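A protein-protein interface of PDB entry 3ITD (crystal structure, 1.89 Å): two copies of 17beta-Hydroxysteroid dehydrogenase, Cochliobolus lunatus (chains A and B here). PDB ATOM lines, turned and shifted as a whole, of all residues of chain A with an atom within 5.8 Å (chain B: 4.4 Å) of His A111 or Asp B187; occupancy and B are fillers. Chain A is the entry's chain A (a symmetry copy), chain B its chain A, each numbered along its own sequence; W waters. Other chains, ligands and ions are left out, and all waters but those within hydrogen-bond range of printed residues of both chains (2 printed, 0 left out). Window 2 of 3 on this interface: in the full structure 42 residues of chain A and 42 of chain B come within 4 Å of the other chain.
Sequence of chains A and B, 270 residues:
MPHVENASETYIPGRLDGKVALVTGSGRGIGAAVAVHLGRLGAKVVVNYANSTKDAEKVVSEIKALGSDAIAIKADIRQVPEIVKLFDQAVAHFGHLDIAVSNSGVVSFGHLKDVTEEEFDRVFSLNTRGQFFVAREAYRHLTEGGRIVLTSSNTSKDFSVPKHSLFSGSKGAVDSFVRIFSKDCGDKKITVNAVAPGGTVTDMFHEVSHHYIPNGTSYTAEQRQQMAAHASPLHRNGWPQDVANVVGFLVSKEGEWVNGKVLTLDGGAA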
ATOM      1  N   PHE A 109      18.800  20.483  -8.164  1.00  0.00           N
ATOM      2  CA  PHE A 109      18.303  19.124  -8.348  1.00  0.00           C
ATOM      3  C   PHE A 109      18.815  18.533  -9.628  1.00  0.00           C
ATOM      4  O   PHE A 109      19.003  19.255 -10.624  1.00  0.00           O
ATOM      5  CB  PHE A 109      16.763  19.108  -8.399  1.00  0.00           C
ATOM      6  CG  PHE A 109      16.127  19.676  -7.152  1.00  0.00           C
ATOM      7  CD1 PHE A 109      15.869  21.056  -7.052  1.00  0.00           C
ATOM      8  CD2 PHE A 109      15.833  18.850  -6.074  1.00  0.00           C
ATOM      9  CE1 PHE A 109      15.302  21.588  -5.887  1.00  0.00           C
ATOM     10  CE2 PHE A 109      15.250  19.379  -4.906  1.00  0.00           C
ATOM     11  CZ  PHE A 109      15.001  20.742  -4.818  1.00  0.00           C
ATOM     12  N   GLY A 110      18.969  17.208  -9.631  1.00  0.00           N
ATOM     13  CA  GLY A 110      19.357  16.475 -10.840  1.00  0.00           C
ATOM     14  C   GLY A 110      19.980  15.126 -10.503  1.00  0.00           C
ATOM     15  O   GLY A 110      20.662  14.983  -9.487  1.00  0.00           O
ATOM     16  N   HIS A 111      19.711  14.128 -11.346  1.00  0.00           N
ATOM     17  CA  HIS A 111      20.317  12.828 -11.197  1.00  0.00           C
ATOM     18  C   HIS A 111      21.853  13.003 -11.348  1.00  0.00           C
ATOM     19  O   HIS A 111      22.324  13.785 -12.178  1.00  0.00           O
ATOM     20  CB  HIS A 111      19.749  11.932 -12.298  1.00  0.00           C
ATOM     21  CG  HIS A 111      20.153  10.497 -12.215  1.00  0.00           C
ATOM     22  ND1 HIS A 111      21.465  10.077 -12.312  1.00  0.00           N
ATOM     23  CD2 HIS A 111      19.401   9.368 -12.138  1.00  0.00           C
ATOM     24  CE1 HIS A 111      21.509   8.754 -12.262  1.00  0.00           C
ATOM     25  NE2 HIS A 111      20.269   8.300 -12.147  1.00  0.00           N
ATOM     26  N   LEU A 112      22.612  12.259 -10.561  1.00  0.00           N
ATOM     27  CA  LEU A 112      24.072  12.256 -10.634  1.00  0.00           C
ATOM     28  C   LEU A 112      24.587  12.254 -12.098  1.00  0.00           C
ATOM     29  O   LEU A 112      25.493  13.020 -12.442  1.00  0.00           O
ATOM     30  CB  LEU A 112      24.605  11.026  -9.885  1.00  0.00           C
ATOM     31  CG  LEU A 112      26.086  10.664 -10.142  1.00  0.00           C
ATOM     32  CD1 LEU A 112      27.013  11.815  -9.669  1.00  0.00           C
ATOM     33  CD2 LEU A 112      26.432   9.329  -9.414  1.00  0.00           C
ATOM     34  N   LYS A 113      24.001  11.409 -12.942  1.00  0.00           N
ATOM     35  CA  LYS A 113      24.508  11.217 -14.312  1.00  0.00           C
ATOM     36  C   LYS A 113      24.575  12.507 -15.141  1.00  0.00           C
ATOM     37  O   LYS A 113      25.354  12.583 -16.102  1.00  0.00           O
ATOM     38  CB  LYS A 113      23.693  10.145 -15.081  1.00  0.00           C
ATOM     39  CG  LYS A 113      22.305  10.584 -15.528  1.00  0.00           C
ATOM     40  CD  LYS A 113      21.483   9.393 -16.040  1.00  0.00           C
ATOM     41  CE  LYS A 113      20.024   9.758 -16.340  1.00  0.00           C
ATOM     42  NZ  LYS A 113      19.926  10.811 -17.382  1.00  0.00           N
ATOM     43  N   ASP A 114      23.758  13.497 -14.758  1.00  0.00           N
ATOM     44  CA  ASP A 114      23.578  14.732 -15.522  1.00  0.00           C
ATOM     45  C   ASP A 114      24.224  15.953 -14.858  1.00  0.00           C
ATOM     46  O   ASP A 114      24.169  17.060 -15.417  1.00  0.00           O
ATOM     47  CB  ASP A 114      22.075  15.041 -15.690  1.00  0.00           C
ATOM     48  CG  ASP A 114      21.341  13.996 -16.492  1.00  0.00           C
ATOM     49  OD1 ASP A 114      21.864  13.585 -17.544  1.00  0.00           O
ATOM     50  OD2 ASP A 114      20.228  13.591 -16.052  1.00  0.00           O
ATOM     51  N   VAL A 115      24.826  15.782 -13.688  1.00  0.00           N
ATOM     52  CA  VAL A 115      25.422  16.927 -12.995  1.00  0.00           C
ATOM     53  C   VAL A 115      26.687  17.397 -13.728  1.00  0.00           C
ATOM     54  O   VAL A 115      27.602  16.590 -13.978  1.00  0.00           O
ATOM     55  CB  VAL A 115      25.739  16.622 -11.502  1.00  0.00           C
ATOM     56  CG1 VAL A 115      26.401  17.845 -10.808  1.00  0.00           C
ATOM     57  CG2 VAL A 115      24.455  16.238 -10.723  1.00  0.00           C
ATOM     58  N   LYS A 163      17.951  12.442  -6.641  1.00  0.00           N
ATOM     59  CA  LYS A 163      18.339  13.533  -7.546  1.00  0.00           C
ATOM     60  C   LYS A 163      18.670  14.800  -6.765  1.00  0.00           C
ATOM     61  O   LYS A 163      18.456  15.916  -7.251  1.00  0.00           O
ATOM     62  CB  LYS A 163      17.250  13.795  -8.615  1.00  0.00           C
ATOM     63  CG  LYS A 163      16.816  12.546  -9.360  1.00  0.00           C
ATOM     64  CD  LYS A 163      15.843  12.856 -10.498  1.00  0.00           C
ATOM     65  CE  LYS A 163      15.571  11.599 -11.304  1.00  0.00           C
ATOM     66  NZ  LYS A 163      14.788  10.590 -10.506  1.00  0.00           N
ATOM     67  N   SER A 165      21.724  14.858  -4.740  1.00  0.00           N
ATOM     68  CA  SER A 165      23.018  14.540  -4.143  1.00  0.00           C
ATOM     69  C   SER A 165      23.929  15.767  -3.951  1.00  0.00           C
ATOM     70  O   SER A 165      24.579  15.918  -2.922  1.00  0.00           O
ATOM     71  CB  SER A 165      23.731  13.440  -4.948  1.00  0.00           C
ATOM     72  OG  SER A 165      24.147  13.915  -6.221  1.00  0.00           O
ATOM     73  N   TYR B 139      29.032   5.618 -12.661  1.00  0.00           N
ATOM     74  CA  TYR B 139      27.640   5.379 -13.008  1.00  0.00           C
ATOM     75  C   TYR B 139      27.455   5.260 -14.516  1.00  0.00           C
ATOM     76  O   TYR B 139      26.745   4.366 -15.006  1.00  0.00           O
ATOM     77  CB  TYR B 139      26.712   6.475 -12.458  1.00  0.00           C
ATOM     78  CG  TYR B 139      25.300   6.281 -12.976  1.00  0.00           C
ATOM     79  CD1 TYR B 139      24.405   5.425 -12.318  1.00  0.00           C
ATOM     80  CD2 TYR B 139      24.882   6.894 -14.161  1.00  0.00           C
ATOM     81  CE1 TYR B 139      23.118   5.207 -12.828  1.00  0.00           C
ATOM     82  CE2 TYR B 139      23.588   6.681 -14.687  1.00  0.00           C
ATOM     83  CZ  TYR B 139      22.722   5.843 -14.013  1.00  0.00           C
ATOM     84  OH  TYR B 139      21.458   5.628 -14.518  1.00  0.00           O
ATOM     85  N   GLU B 144      25.382  -3.123 -15.336  1.00  0.00           N
ATOM     86  CA  GLU B 144      24.323  -3.309 -14.333  1.00  0.00           C
ATOM     87  C   GLU B 144      24.750  -4.233 -13.197  1.00  0.00           C
ATOM     88  O   GLU B 144      25.404  -5.235 -13.422  1.00  0.00           O
ATOM     89  CB  GLU B 144      23.063  -3.874 -14.989  1.00  0.00           C
ATOM     90  CG  GLU B 144      22.448  -2.927 -16.009  1.00  0.00           C
ATOM     91  CD  GLU B 144      21.122  -2.327 -15.550  1.00  0.00           C
ATOM     92  OE1 GLU B 144      20.469  -2.894 -14.628  1.00  0.00           O
ATOM     93  OE2 GLU B 144      20.721  -1.301 -16.150  1.00  0.00           O
ATOM     94  N   ASP B 184      20.073   7.291  -6.852  1.00  0.00           N
ATOM     95  CA  ASP B 184      20.165   7.490  -8.303  1.00  0.00           C
ATOM     96  C   ASP B 184      20.759   6.256  -9.030  1.00  0.00           C
ATOM     97  O   ASP B 184      20.269   5.845 -10.088  1.00  0.00           O
ATOM     98  CB  ASP B 184      21.038   8.726  -8.618  1.00  0.00           C
ATOM     99  CG  ASP B 184      20.430  10.051  -8.128  1.00  0.00           C
ATOM    100  OD1 ASP B 184      19.269  10.100  -7.645  1.00  0.00           O
ATOM    101  OD2 ASP B 184      21.147  11.069  -8.235  1.00  0.00           O
ATOM    102  N   CYS B 185      21.790   5.651  -8.446  1.00  0.00           N
ATOM    103  CA  CYS B 185      22.487   4.543  -9.100  1.00  0.00           C
ATOM    104  C   CYS B 185      21.724   3.222  -9.031  1.00  0.00           C
ATOM    105  O   CYS B 185      22.072   2.265  -9.717  1.00  0.00           O
ATOM    106  CB  CYS B 185      23.894   4.370  -8.501  1.00  0.00           C
ATOM    107  SG  CYS B 185      24.998   5.779  -8.749  1.00  0.00           S
ATOM    108  N   GLY B 186      20.689   3.171  -8.195  1.00  0.00           N
ATOM    109  CA  GLY B 186      19.778   2.023  -8.132  1.00  0.00           C
ATOM    110  C   GLY B 186      19.122   1.703  -9.474  1.00  0.00           C
ATOM    111  O   GLY B 186      18.719   0.558  -9.722  1.00  0.00           O
ATOM    112  N   ASP B 187      18.983   2.701 -10.349  1.00  0.00           N
ATOM    113  CA  ASP B 187      18.354   2.433 -11.627  1.00  0.00           C
ATOM    114  C   ASP B 187      19.237   1.591 -12.588  1.00  0.00           C
ATOM    115  O   ASP B 187      18.751   1.093 -13.615  1.00  0.00           O
ATOM    116  CB  ASP B 187      17.738   3.709 -12.250  1.00  0.00           C
ATOM    117  CG  ASP B 187      18.777   4.710 -12.696  1.00  0.00           C
ATOM    118  OD1 ASP B 187      19.879   4.258 -13.084  1.00  0.00           O
ATOM    119  OD2 ASP B 187      18.490   5.946 -12.672  1.00  0.00           O
ATOM    120  N   LYS B 188      20.511   1.422 -12.230  1.00  0.00           N
ATOM    121  CA  LYS B 188      21.404   0.426 -12.848  1.00  0.00           C
ATOM    122  C   LYS B 188      21.769  -0.721 -11.875  1.00  0.00           C
ATOM    123  O   LYS B 188      22.657  -1.539 -12.162  1.00  0.00           O
ATOM    124  CB  LYS B 188      22.672   1.094 -13.400  1.00  0.00           C
ATOM    125  CG  LYS B 188      22.421   1.983 -14.633  1.00  0.00           C
ATOM    126  CD  LYS B 188      23.723   2.616 -15.164  1.00  0.00           C
ATOM    127  CE  LYS B 188      24.518   1.675 -16.035  1.00  0.00           C
ATOM    128  NZ  LYS B 188      25.772   2.342 -16.611  1.00  0.00           N
ATOM    129  N   LYS B 189      21.059  -0.785 -10.739  1.00  0.00           N
ATOM    130  CA  LYS B 189      21.335  -1.760  -9.667  1.00  0.00           C
ATOM    131  C   LYS B 189      22.794  -1.694  -9.173  1.00  0.00           C
ATOM    132  O   LYS B 189      23.370  -2.708  -8.769  1.00  0.00           O
ATOM    133  CB  LYS B 189      20.998  -3.196 -10.083  1.00  0.00           C
ATOM    134  CG  LYS B 189      19.555  -3.444 -10.638  1.00  0.00           C
ATOM    135  CD  LYS B 189      18.476  -2.798  -9.818  1.00  0.00           C
ATOM    136  CE  LYS B 189      17.153  -2.677 -10.605  1.00  0.00           C
ATOM    137  NZ  LYS B 189      16.408  -3.917 -10.464  1.00  0.00           N
HETATM  138  O   HOH W   1      21.694  13.433  -7.433  1.00  0.00           O
HETATM  139  O   HOH W   2      17.007   9.078  -9.128  1.00  0.00           O
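Water W1 lies within hydrogen-bond range of OD2 of Asp B184 (2.6 Å), O of Gly A110 (2.8 Å), OG of Ser A165 (2.8 Å) and N of Leu A112 (3.5 Å).
Water W2 bridges the side-chain carboxylate of Asp B184 (2.9 Å) and the side-chain amino group of Lys A163 (3.0 Å).
The side-chain carboxylate (OD1) of Asp B187 sits at hydrogen-bond distance from the side-chain hydroxyl (OH) of Tyr B139, 2.5 Å away.
The backbone carbonyl oxygen (O) of Tyr B139 lies within hydrogen-bond range of the side-chain amino group (NZ) of Lys B188.
OD2 of Asp A114 lies within salt-bridge range of NZ of Lys A113, 3.1 Å away.
The backbone NH of Gly A110 is in hydrogen-bond range of the backbone carbonyl oxygen of Lys A163, at 2.8 Å.
The backbone NH of Lys A113 sits at hydrogen-bond distance from a ring nitrogen (ND1) of His A111 (2.9 Å).
No position is printed for both chains.
Of the 7 pairs that touch across the chains among the printed residues, none has its exchanged pair printed and touching as well.
OD2 of Asp B187 is in hydrogen-bond range of NE2 of His A111.
O of Asp B184 lies within hydrogen-bond range of NE2 of His A111, 3.2 Å away.
The side-chain carboxylate (OD2) of Asp B184 is in hydrogen-bond range of the backbone NH (N) of Leu A112, at 3.0 Å.
The side-chain carboxylate of Asp B184 is in hydrogen-bond range of the backbone NH of Lys A163, at 2.9 Å.
His A111 touches just these residues of chain B: Tyr B139 (3.6 Å), Asp B184 (3.2 Å) and Asp B187 (3.0 Å).
Asp A114 touches none of the printed residues of chain B.
Of the printed residues of chain B, Lys A163 touches Asp B184 (2.9 Å).
Of the printed residues of chain A, Asp B184 touches His A111 (3.2 Å), Leu A112 (3.0 Å) and Lys A163 (2.9 Å).
Of the printed residues of chain A, Cys B185 touches Leu A112 (3.9 Å).
Of chain A, only His A111 comes within 4 Å of Asp B187.
The nearest printed residue of chain B that does not touch His A111 is Cys B185 (4.8 Å).
The nearest printed residue of chain A that does not touch Cys B185 is His A111 (4.8 Å).
Among the printed residues, pairs that only touch across the chains: His A111 with Tyr B139, Leu A112 with Cys B185 and Lys A113 with Tyr B139.
Of the 8 printed residues of chain B, 4 touch a printed residue of chain A.
Hydrophobic or aromatic side chains of chain B that line the printed part of chain A: Tyr B139.
Along chain B the printed residues that touch a printed residue of chain A span positions 139 to 187.
Of the 9 printed residues of chain A, 4 touch a printed residue of chain B.
Hydrophobic or aromatic side chains of chain A that line the printed part of chain B: His A111 and Leu A112.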
